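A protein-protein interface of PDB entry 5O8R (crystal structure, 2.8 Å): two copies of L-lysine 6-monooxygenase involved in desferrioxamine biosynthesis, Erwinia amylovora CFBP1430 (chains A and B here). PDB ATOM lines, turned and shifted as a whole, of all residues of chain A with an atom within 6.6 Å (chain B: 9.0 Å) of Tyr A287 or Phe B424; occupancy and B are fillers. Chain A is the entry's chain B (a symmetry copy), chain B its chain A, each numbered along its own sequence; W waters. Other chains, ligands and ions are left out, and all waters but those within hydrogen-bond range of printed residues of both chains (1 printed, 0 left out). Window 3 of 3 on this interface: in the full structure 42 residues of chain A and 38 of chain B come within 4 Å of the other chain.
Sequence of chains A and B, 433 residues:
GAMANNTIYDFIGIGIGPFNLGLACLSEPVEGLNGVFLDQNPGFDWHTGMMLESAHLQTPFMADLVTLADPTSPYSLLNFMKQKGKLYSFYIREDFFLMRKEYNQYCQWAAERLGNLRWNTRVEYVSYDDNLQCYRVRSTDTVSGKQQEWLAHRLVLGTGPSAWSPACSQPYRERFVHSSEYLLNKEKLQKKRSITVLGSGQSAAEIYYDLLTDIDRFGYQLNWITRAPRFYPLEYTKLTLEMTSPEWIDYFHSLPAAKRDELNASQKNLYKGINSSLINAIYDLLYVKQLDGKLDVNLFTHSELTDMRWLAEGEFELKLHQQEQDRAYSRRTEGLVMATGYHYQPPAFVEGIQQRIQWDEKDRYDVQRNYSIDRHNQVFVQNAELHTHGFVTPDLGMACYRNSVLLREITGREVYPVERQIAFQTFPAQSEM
The side-chain carboxylate of Asp A284 is in salt-bridge range of the side-chain amino group of Lys B238 (3.0 Å).
O of Leu A299 is in hydrogen-bond range of N of Thr B426, 3.1 Å away.
No position is printed for both chains.
Among the printed residues, pairs that only touch across the chains: Tyr A283 with Lys B238, Tyr A283 with Glu B242, Tyr A283 with Phe B424, Leu A286 with Phe B424, Tyr A287 with Phe B424, Gln A290 with Phe B424 and Leu A299 with Gln B425.
Of chain B, only Phe B424 comes within 4 Å of Leu A286.
Of chain B, only Phe B424 (3.8 Å) comes within 4 Å of Tyr A287.
Of the printed residues of chain A, Lys B238 touches Tyr A283 and Asp A284.
Printed residues of chain A within 4 Å of Glu B242: Tyr A283.
Printed residues of chain A within 4 Å of Phe B424: Tyr A283, Leu A286, Tyr A287 and Gln A290.
The nearest printed residue of chain A that does not touch Glu B242 is Leu A286 (6.4 Å).
The side-chain amide nitrogen (NE2) of Gln B425 lies within hydrogen-bond range of the backbone carbonyl oxygen (O) of Leu B239, at 2.9 Å.
O of Glu B242 sits at hydrogen-bond distance from OG of Ser B245 (2.5 Å).
N of Phe B424 sits at hydrogen-bond distance from OE2 of Glu B242 (2.9 Å).
The side-chain carboxylate (OE1) of Glu B242 lies within hydrogen-bond range of the side-chain amide nitrogen (NE2) of Gln B425 (2.5 Å).
Of the 15 printed residues of chain B, 5 touch a printed residue of chain A.
Along chain B the printed residues that touch a printed residue of chain A span positions 238 to 426.
Of the 15 printed residues of chain A, 6 touch a printed residue of chain B.
Printed residues of chain A that touch a printed residue of chain B: Tyr A283, Asp A284, Leu A286, Tyr A287, Gln A290 and Leu A299.
Hydrophobic or aromatic side chains of chain A that line the printed part of chain B: Tyr A283, Leu A286 and Leu A299.
Water W1 lies within hydrogen-bond range of the side-chain hydroxyl of Tyr A283 (2.6 Å), the side-chain carboxylate of Glu B242 (2.6 Å) and the backbone carbonyl oxygen of Ile B422 (3.1 Å).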
ATOM      1  N   ILE A 282       8.932 -18.326  -0.745  1.00  0.00           N
ATOM      2  CA  ILE A 282       8.199 -18.084  -1.946  1.00  0.00           C
ATOM      3  C   ILE A 282       9.017 -17.199  -2.852  1.00  0.00           C
ATOM      4  O   ILE A 282       9.247 -17.528  -4.008  1.00  0.00           O
ATOM      5  CB  ILE A 282       6.858 -17.433  -1.631  1.00  0.00           C
ATOM      6  CG1 ILE A 282       5.919 -18.461  -1.009  1.00  0.00           C
ATOM      7  CG2 ILE A 282       6.212 -16.913  -2.896  1.00  0.00           C
ATOM      8  CD1 ILE A 282       4.696 -17.848  -0.359  1.00  0.00           C
ATOM      9  N   TYR A 283       9.483 -16.074  -2.327  1.00  0.00           N
ATOM     10  CA  TYR A 283      10.368 -15.186  -3.113  1.00  0.00           C
ATOM     11  C   TYR A 283      11.591 -15.917  -3.658  1.00  0.00           C
ATOM     12  O   TYR A 283      11.867 -15.818  -4.832  1.00  0.00           O
ATOM     13  CB  TYR A 283      10.802 -13.966  -2.317  1.00  0.00           C
ATOM     14  CG  TYR A 283      11.607 -13.013  -3.138  1.00  0.00           C
ATOM     15  CD1 TYR A 283      12.938 -13.261  -3.379  1.00  0.00           C
ATOM     16  CD2 TYR A 283      11.042 -11.850  -3.671  1.00  0.00           C
ATOM     17  CE1 TYR A 283      13.685 -12.377  -4.147  1.00  0.00           C
ATOM     18  CE2 TYR A 283      11.783 -10.975  -4.455  1.00  0.00           C
ATOM     19  CZ  TYR A 283      13.095 -11.257  -4.687  1.00  0.00           C
ATOM     20  OH  TYR A 283      13.897 -10.465  -5.437  1.00  0.00           O
ATOM     21  N   ASP A 284      12.294 -16.666  -2.816  1.00  0.00           N
ATOM     22  CA  ASP A 284      13.454 -17.395  -3.268  1.00  0.00           C
ATOM     23  C   ASP A 284      13.045 -18.356  -4.346  1.00  0.00           C
ATOM     24  O   ASP A 284      13.751 -18.494  -5.341  1.00  0.00           O
ATOM     25  CB  ASP A 284      14.170 -18.141  -2.147  1.00  0.00           C
ATOM     26  CG  ASP A 284      14.894 -17.206  -1.164  1.00  0.00           C
ATOM     27  OD1 ASP A 284      15.096 -15.978  -1.429  1.00  0.00           O
ATOM     28  OD2 ASP A 284      15.253 -17.727  -0.086  1.00  0.00           O
ATOM     29  N   LEU A 285      11.894 -18.989  -4.210  1.00  0.00           N
ATOM     30  CA  LEU A 285      11.447 -19.878  -5.289  1.00  0.00           C
ATOM     31  C   LEU A 285      11.085 -19.129  -6.594  1.00  0.00           C
ATOM     32  O   LEU A 285      11.368 -19.624  -7.662  1.00  0.00           O
ATOM     33  CB  LEU A 285      10.286 -20.772  -4.853  1.00  0.00           C
ATOM     34  CG  LEU A 285      10.091 -22.042  -5.695  1.00  0.00           C
ATOM     35  CD1 LEU A 285      11.331 -22.937  -5.844  1.00  0.00           C
ATOM     36  CD2 LEU A 285       8.978 -22.838  -5.056  1.00  0.00           C
ATOM     37  N   LEU A 286      10.492 -17.947  -6.529  1.00  0.00           N
ATOM     38  CA  LEU A 286      10.263 -17.218  -7.747  1.00  0.00           C
ATOM     39  C   LEU A 286      11.618 -16.908  -8.406  1.00  0.00           C
ATOM     40  O   LEU A 286      11.800 -17.082  -9.590  1.00  0.00           O
ATOM     41  CB  LEU A 286       9.500 -15.935  -7.450  1.00  0.00           C
ATOM     42  CG  LEU A 286       8.075 -16.118  -6.970  1.00  0.00           C
ATOM     43  CD1 LEU A 286       7.389 -14.845  -6.474  1.00  0.00           C
ATOM     44  CD2 LEU A 286       7.264 -16.718  -8.096  1.00  0.00           C
ATOM     45  N   TYR A 287      12.575 -16.467  -7.624  1.00  0.00           N
ATOM     46  CA  TYR A 287      13.910 -16.196  -8.119  1.00  0.00           C
ATOM     47  C   TYR A 287      14.515 -17.443  -8.785  1.00  0.00           C
ATOM     48  O   TYR A 287      15.065 -17.358  -9.870  1.00  0.00           O
ATOM     49  CB  TYR A 287      14.795 -15.724  -6.938  1.00  0.00           C
ATOM     50  CG  TYR A 287      16.173 -15.293  -7.320  1.00  0.00           C
ATOM     51  CD1 TYR A 287      17.171 -16.251  -7.540  1.00  0.00           C
ATOM     52  CD2 TYR A 287      16.471 -13.950  -7.471  1.00  0.00           C
ATOM     53  CE1 TYR A 287      18.435 -15.895  -7.895  1.00  0.00           C
ATOM     54  CE2 TYR A 287      17.732 -13.562  -7.834  1.00  0.00           C
ATOM     55  CZ  TYR A 287      18.718 -14.548  -8.044  1.00  0.00           C
ATOM     56  OH  TYR A 287      19.988 -14.226  -8.425  1.00  0.00           O
ATOM     57  N   VAL A 288      14.419 -18.602  -8.150  1.00  0.00           N
ATOM     58  CA  VAL A 288      15.022 -19.780  -8.756  1.00  0.00           C
ATOM     59  C   VAL A 288      14.315 -20.205 -10.032  1.00  0.00           C
ATOM     60  O   VAL A 288      14.950 -20.507 -11.024  1.00  0.00           O
ATOM     61  CB  VAL A 288      15.063 -20.954  -7.806  1.00  0.00           C
ATOM     62  CG1 VAL A 288      15.704 -22.139  -8.493  1.00  0.00           C
ATOM     63  CG2 VAL A 288      15.937 -20.607  -6.617  1.00  0.00           C
ATOM     64  N   LYS A 289      12.995 -20.250  -9.991  1.00  0.00           N
ATOM     65  CA  LYS A 289      12.239 -20.598 -11.157  1.00  0.00           C
ATOM     66  C   LYS A 289      12.562 -19.662 -12.306  1.00  0.00           C
ATOM     67  O   LYS A 289      12.626 -20.132 -13.430  1.00  0.00           O
ATOM     68  CB  LYS A 289      10.749 -20.555 -10.881  1.00  0.00           C
ATOM     69  CG  LYS A 289      10.180 -21.670 -10.001  1.00  0.00           C
ATOM     70  CD  LYS A 289      10.564 -23.060 -10.456  1.00  0.00           C
ATOM     71  CE  LYS A 289       9.722 -24.074  -9.727  1.00  0.00           C
ATOM     72  NZ  LYS A 289      10.475 -25.340  -9.500  1.00  0.00           N
ATOM     73  N   GLN A 290      12.767 -18.369 -12.049  1.00  0.00           N
ATOM     74  CA  GLN A 290      13.030 -17.378 -13.124  1.00  0.00           C
ATOM     75  C   GLN A 290      14.331 -17.607 -13.847  1.00  0.00           C
ATOM     76  O   GLN A 290      14.553 -17.105 -14.928  1.00  0.00           O
ATOM     77  CB  GLN A 290      13.048 -15.917 -12.611  1.00  0.00           C
ATOM     78  CG  GLN A 290      13.624 -14.869 -13.604  1.00  0.00           C
ATOM     79  CD  GLN A 290      12.875 -13.552 -13.571  1.00  0.00           C
ATOM     80  OE1 GLN A 290      12.307 -13.164 -12.550  1.00  0.00           O
ATOM     81  NE2 GLN A 290      12.823 -12.870 -14.723  1.00  0.00           N
ATOM     82  N   LEU A 291      15.222 -18.343 -13.242  1.00  0.00           N
ATOM     83  CA  LEU A 291      16.492 -18.595 -13.889  1.00  0.00           C
ATOM     84  C   LEU A 291      16.360 -19.306 -15.220  1.00  0.00           C
ATOM     85  O   LEU A 291      17.127 -19.004 -16.121  1.00  0.00           O
ATOM     86  CB  LEU A 291      17.388 -19.411 -12.986  1.00  0.00           C
ATOM     87  CG  LEU A 291      17.809 -18.721 -11.700  1.00  0.00           C
ATOM     88  CD1 LEU A 291      18.510 -19.690 -10.765  1.00  0.00           C
ATOM     89  CD2 LEU A 291      18.710 -17.542 -12.016  1.00  0.00           C
ATOM     90  N   ASP A 292      15.412 -20.236 -15.341  1.00  0.00           N
ATOM     91  CA  ASP A 292      15.121 -20.915 -16.631  1.00  0.00           C
ATOM     92  C   ASP A 292      14.489 -20.047 -17.721  1.00  0.00           C
ATOM     93  O   ASP A 292      14.828 -20.170 -18.866  1.00  0.00           O
ATOM     94  CB  ASP A 292      14.252 -22.147 -16.427  1.00  0.00           C
ATOM     95  CG  ASP A 292      14.991 -23.246 -15.724  1.00  0.00           C
ATOM     96  OD1 ASP A 292      16.239 -23.244 -15.798  1.00  0.00           O
ATOM     97  OD2 ASP A 292      14.340 -24.104 -15.088  1.00  0.00           O
ATOM     98  N   LEU A 295       8.763 -16.203 -15.884  1.00  0.00           N
ATOM     99  CA  LEU A 295       7.740 -17.008 -15.256  1.00  0.00           C
ATOM    100  C   LEU A 295       6.442 -16.388 -15.546  1.00  0.00           C
ATOM    101  O   LEU A 295       6.297 -15.135 -15.492  1.00  0.00           O
ATOM    102  CB  LEU A 295       7.825 -16.992 -13.732  1.00  0.00           C
ATOM    103  CG  LEU A 295       9.121 -17.420 -13.140  1.00  0.00           C
ATOM    104  CD1 LEU A 295       9.011 -17.197 -11.650  1.00  0.00           C
ATOM    105  CD2 LEU A 295       9.373 -18.868 -13.546  1.00  0.00           C
ATOM    106  N   VAL A 297       3.771 -15.595 -13.862  1.00  0.00           N
ATOM    107  CA  VAL A 297       3.182 -15.323 -12.553  1.00  0.00           C
ATOM    108  C   VAL A 297       2.744 -13.902 -12.504  1.00  0.00           C
ATOM    109  O   VAL A 297       3.369 -13.059 -13.094  1.00  0.00           O
ATOM    110  CB  VAL A 297       4.168 -15.552 -11.389  1.00  0.00           C
ATOM    111  CG1 VAL A 297       4.537 -17.026 -11.254  1.00  0.00           C
ATOM    112  CG2 VAL A 297       5.436 -14.708 -11.552  1.00  0.00           C
ATOM    113  N   ASN A 298       1.650 -13.638 -11.818  1.00  0.00           N
ATOM    114  CA  ASN A 298       1.218 -12.278 -11.556  1.00  0.00           C
ATOM    115  C   ASN A 298       0.833 -12.184 -10.104  1.00  0.00           C
ATOM    116  O   ASN A 298       0.297 -13.135  -9.513  1.00  0.00           O
ATOM    117  CB  ASN A 298       0.023 -11.926 -12.439  1.00  0.00           C
ATOM    118  CG  ASN A 298       0.361 -11.967 -13.915  1.00  0.00           C
ATOM    119  OD1 ASN A 298       0.099 -12.970 -14.588  1.00  0.00           O
ATOM    120  ND2 ASN A 298       1.001 -10.908 -14.414  1.00  0.00           N
ATOM    121  N   LEU A 299       1.122 -11.040  -9.506  1.00  0.00           N
ATOM    122  CA  LEU A 299       0.956 -10.891  -8.067  1.00  0.00           C
ATOM    123  C   LEU A 299       0.381  -9.531  -7.819  1.00  0.00           C
ATOM    124  O   LEU A 299       1.073  -8.547  -8.023  1.00  0.00           O
ATOM    125  CB  LEU A 299       2.319 -11.086  -7.351  1.00  0.00           C
ATOM    126  CG  LEU A 299       2.773 -12.563  -7.185  1.00  0.00           C
ATOM    127  CD1 LEU A 299       3.851 -13.036  -8.132  1.00  0.00           C
ATOM    128  CD2 LEU A 299       3.276 -12.789  -5.779  1.00  0.00           C
ATOM    129  N   LYS B 238      10.775 -10.445   2.054  1.00  0.00           N
ATOM    130  CA  LYS B 238      11.359 -10.135   0.760  1.00  0.00           C
ATOM    131  C   LYS B 238      10.372  -9.663  -0.244  1.00  0.00           C
ATOM    132  O   LYS B 238      10.691  -8.785  -1.048  1.00  0.00           O
ATOM    133  CB  LYS B 238      12.075 -11.340   0.225  1.00  0.00           C
ATOM    134  CG  LYS B 238      13.271 -11.708   1.072  1.00  0.00           C
ATOM    135  CD  LYS B 238      13.930 -12.920   0.496  1.00  0.00           C
ATOM    136  CE  LYS B 238      15.354 -13.040   0.930  1.00  0.00           C
ATOM    137  NZ  LYS B 238      15.662 -14.478   1.152  1.00  0.00           N
ATOM    138  N   LEU B 239       9.163 -10.221  -0.193  1.00  0.00           N
ATOM    139  CA  LEU B 239       8.038  -9.631  -0.951  1.00  0.00           C
ATOM    140  C   LEU B 239       7.832  -8.163  -0.651  1.00  0.00           C
ATOM    141  O   LEU B 239       7.721  -7.383  -1.590  1.00  0.00           O
ATOM    142  CB  LEU B 239       6.723 -10.406  -0.822  1.00  0.00           C
ATOM    143  CG  LEU B 239       6.625 -11.695  -1.692  1.00  0.00           C
ATOM    144  CD1 LEU B 239       5.258 -12.343  -1.494  1.00  0.00           C
ATOM    145  CD2 LEU B 239       6.895 -11.467  -3.173  1.00  0.00           C
ATOM    146  N   GLU B 242      10.340  -5.497  -2.268  1.00  0.00           N
ATOM    147  CA  GLU B 242      10.001  -5.056  -3.643  1.00  0.00           C
ATOM    148  C   GLU B 242       9.374  -3.680  -3.666  1.00  0.00           C
ATOM    149  O   GLU B 242       9.498  -2.931  -4.625  1.00  0.00           O
ATOM    150  CB  GLU B 242       9.105  -6.061  -4.354  1.00  0.00           C
ATOM    151  CG  GLU B 242       9.872  -7.301  -4.777  1.00  0.00           C
ATOM    152  CD  GLU B 242       9.070  -8.225  -5.642  1.00  0.00           C
ATOM    153  OE1 GLU B 242       7.811  -8.254  -5.501  1.00  0.00           O
ATOM    154  OE2 GLU B 242       9.718  -8.920  -6.455  1.00  0.00           O
ATOM    155  N   MET B 243       8.765  -3.292  -2.578  1.00  0.00           N
ATOM    156  CA  MET B 243       8.262  -1.964  -2.533  1.00  0.00           C
ATOM    157  C   MET B 243       9.359  -0.905  -2.381  1.00  0.00           C
ATOM    158  O   MET B 243       9.062   0.288  -2.383  1.00  0.00           O
ATOM    159  CB  MET B 243       7.297  -1.817  -1.388  1.00  0.00           C
ATOM    160  CG  MET B 243       6.132  -2.778  -1.339  1.00  0.00           C
ATOM    161  SD  MET B 243       5.204  -2.182   0.088  1.00  0.00           S
ATOM    162  CE  MET B 243       3.530  -2.367  -0.540  1.00  0.00           C
ATOM    163  N   SER B 245      11.634  -0.102  -4.603  1.00  0.00           N
ATOM    164  CA  SER B 245      12.212  -0.343  -5.898  1.00  0.00           C
ATOM    165  C   SER B 245      11.632   0.651  -6.864  1.00  0.00           C
ATOM    166  O   SER B 245      10.466   1.073  -6.705  1.00  0.00           O
ATOM    167  CB  SER B 245      11.985  -1.798  -6.375  1.00  0.00           C
ATOM    168  OG  SER B 245      10.616  -2.017  -6.646  1.00  0.00           O
ATOM    169  N   GLU B 247      10.119   0.496  -9.528  1.00  0.00           N
ATOM    170  CA  GLU B 247       8.751   0.129  -9.946  1.00  0.00           C
ATOM    171  C   GLU B 247       7.761   0.661  -8.924  1.00  0.00           C
ATOM    172  O   GLU B 247       6.809   1.346  -9.261  1.00  0.00           O
ATOM    173  CB  GLU B 247       8.597  -1.400 -10.124  1.00  0.00           C
ATOM    174  CG  GLU B 247       9.834  -2.123 -10.692  1.00  0.00           C
ATOM    175  CD  GLU B 247       9.566  -3.448 -11.415  1.00  0.00           C
ATOM    176  OE1 GLU B 247       8.406  -3.921 -11.590  1.00  0.00           O
ATOM    177  OE2 GLU B 247      10.586  -4.046 -11.809  1.00  0.00           O
ATOM    178  N   ARG B 420      14.515  -1.385 -13.865  1.00  0.00           N
ATOM    179  CA  ARG B 420      13.012  -1.377 -13.727  1.00  0.00           C
ATOM    180  C   ARG B 420      12.330  -2.731 -14.010  1.00  0.00           C
ATOM    181  O   ARG B 420      11.091  -2.799 -14.031  1.00  0.00           O
ATOM    182  CB  ARG B 420      12.370  -0.291 -14.591  1.00  0.00           C
ATOM    183  CG  ARG B 420      12.859   1.100 -14.261  1.00  0.00           C
ATOM    184  CD  ARG B 420      12.124   2.223 -14.994  1.00  0.00           C
ATOM    185  NE  ARG B 420      12.037   3.409 -14.116  1.00  0.00           N
ATOM    186  CZ  ARG B 420      12.952   4.384 -13.988  1.00  0.00           C
ATOM    187  NH1 ARG B 420      14.073   4.399 -14.714  1.00  0.00           N
ATOM    188  NH2 ARG B 420      12.733   5.377 -13.128  1.00  0.00           N
ATOM    189  N   GLN B 421      13.152  -3.785 -14.202  1.00  0.00           N
ATOM    190  CA  GLN B 421      12.726  -5.183 -14.470  1.00  0.00           C
ATOM    191  C   GLN B 421      12.980  -6.103 -13.256  1.00  0.00           C
ATOM    192  O   GLN B 421      13.549  -7.203 -13.419  1.00  0.00           O
ATOM    193  CB  GLN B 421      13.516  -5.774 -15.662  1.00  0.00           C
ATOM    194  CG  GLN B 421      13.532  -4.949 -16.938  1.00  0.00           C
ATOM    195  CD  GLN B 421      12.218  -5.001 -17.702  1.00  0.00           C
ATOM    196  OE1 GLN B 421      11.160  -4.582 -17.203  1.00  0.00           O
ATOM    197  NE2 GLN B 421      12.282  -5.506 -18.933  1.00  0.00           N
ATOM    198  N   ILE B 422      12.564  -5.657 -12.060  1.00  0.00           N
ATOM    199  CA  ILE B 422      12.937  -6.284 -10.762  1.00  0.00           C
ATOM    200  C   ILE B 422      11.821  -7.094 -10.101  1.00  0.00           C
ATOM    201  O   ILE B 422      11.953  -8.286  -9.801  1.00  0.00           O
ATOM    202  CB  ILE B 422      13.359  -5.173  -9.774  1.00  0.00           C
ATOM    203  CG1 ILE B 422      14.702  -4.578 -10.186  1.00  0.00           C
ATOM    204  CG2 ILE B 422      13.445  -5.688  -8.344  1.00  0.00           C
ATOM    205  CD1 ILE B 422      15.854  -5.584 -10.328  1.00  0.00           C
ATOM    206  N   ALA B 423      10.729  -6.390  -9.858  1.00  0.00           N
ATOM    207  CA  ALA B 423       9.656  -6.869  -9.055  1.00  0.00           C
ATOM    208  C   ALA B 423       8.849  -7.899  -9.792  1.00  0.00           C
ATOM    209  O   ALA B 423       8.381  -7.658 -10.885  1.00  0.00           O
ATOM    210  CB  ALA B 423       8.759  -5.714  -8.661  1.00  0.00           C
ATOM    211  N   PHE B 424       8.657  -9.032  -9.146  1.00  0.00           N
ATOM    212  CA  PHE B 424       7.634  -9.975  -9.535  1.00  0.00           C
ATOM    213  C   PHE B 424       6.216  -9.403  -9.376  1.00  0.00           C
ATOM    214  O   PHE B 424       5.325  -9.651 -10.178  1.00  0.00           O
ATOM    215  CB  PHE B 424       7.775 -11.184  -8.668  1.00  0.00           C
ATOM    216  CG  PHE B 424       9.056 -11.869  -8.843  1.00  0.00           C
ATOM    217  CD1 PHE B 424       9.266 -12.647  -9.934  1.00  0.00           C
ATOM    218  CD2 PHE B 424      10.058 -11.727  -7.941  1.00  0.00           C
ATOM    219  CE1 PHE B 424      10.454 -13.318 -10.115  1.00  0.00           C
ATOM    220  CE2 PHE B 424      11.271 -12.386  -8.111  1.00  0.00           C
ATOM    221  CZ  PHE B 424      11.469 -13.190  -9.202  1.00  0.00           C
ATOM    222  N   GLN B 425       5.981  -8.648  -8.323  1.00  0.00           N
ATOM    223  CA  GLN B 425       4.668  -8.056  -8.137  1.00  0.00           C
ATOM    224  C   GLN B 425       4.427  -7.057  -9.208  1.00  0.00           C
ATOM    225  O   GLN B 425       5.356  -6.379  -9.621  1.00  0.00           O
ATOM    226  CB  GLN B 425       4.603  -7.310  -6.834  1.00  0.00           C
ATOM    227  CG  GLN B 425       4.618  -8.223  -5.654  1.00  0.00           C
ATOM    228  CD  GLN B 425       4.795  -7.479  -4.378  1.00  0.00           C
ATOM    229  OE1 GLN B 425       3.826  -6.911  -3.832  1.00  0.00           O
ATOM    230  NE2 GLN B 425       6.022  -7.479  -3.879  1.00  0.00           N
ATOM    231  N   THR B 426       3.188  -6.965  -9.658  1.00  0.00           N
ATOM    232  CA  THR B 426       2.708  -5.732 -10.275  1.00  0.00           C
ATOM    233  C   THR B 426       2.030  -4.852  -9.218  1.00  0.00           C
ATOM    234  O   THR B 426       1.180  -5.328  -8.439  1.00  0.00           O
ATOM    235  CB  THR B 426       1.720  -6.046 -11.384  1.00  0.00           C
ATOM    236  OG1 THR B 426       2.289  -7.048 -12.226  1.00  0.00           O
ATOM    237  CG2 THR B 426       1.404  -4.808 -12.197  1.00  0.00           C
ATOM    238  N   PHE B 427       2.414  -3.582  -9.162  1.00  0.00           N
ATOM    239  CA  PHE B 427       1.841  -2.702  -8.135  1.00  0.00           C
ATOM    240  C   PHE B 427       0.563  -1.930  -8.459  1.00  0.00           C
ATOM    241  O   PHE B 427      -0.308  -1.806  -7.584  1.00  0.00           O
ATOM    242  CB  PHE B 427       2.891  -1.737  -7.626  1.00  0.00           C
ATOM    243  CG  PHE B 427       4.041  -2.424  -6.995  1.00  0.00           C
ATOM    244  CD1 PHE B 427       3.856  -3.150  -5.813  1.00  0.00           C
ATOM    245  CD2 PHE B 427       5.291  -2.389  -7.593  1.00  0.00           C
ATOM    246  CE1 PHE B 427       4.904  -3.818  -5.229  1.00  0.00           C
ATOM    247  CE2 PHE B 427       6.346  -3.048  -7.014  1.00  0.00           C
ATOM    248  CZ  PHE B 427       6.154  -3.765  -5.827  1.00  0.00           C
ATOM    249  N   GLN B 430      -3.948  -3.269 -13.301  1.00  0.00           N
ATOM    250  CA  GLN B 430      -3.530  -3.621 -14.657  1.00  0.00           C
ATOM    251  C   GLN B 430      -4.484  -4.690 -15.131  1.00  0.00           C
ATOM    252  O   GLN B 430      -4.769  -5.612 -14.388  1.00  0.00           O
ATOM    253  CB  GLN B 430      -2.114  -4.185 -14.669  1.00  0.00           C
ATOM    254  CG  GLN B 430      -1.745  -4.897 -15.972  1.00  0.00           C
ATOM    255  CD  GLN B 430      -0.291  -5.319 -16.025  1.00  0.00           C
ATOM    256  OE1 GLN B 430       0.590  -4.511 -15.715  1.00  0.00           O
ATOM    257  NE2 GLN B 430      -0.027  -6.582 -16.434  1.00  0.00           N
HETATM  258  O   HOH W   1      12.276  -9.004  -6.815  1.00  0.00           O
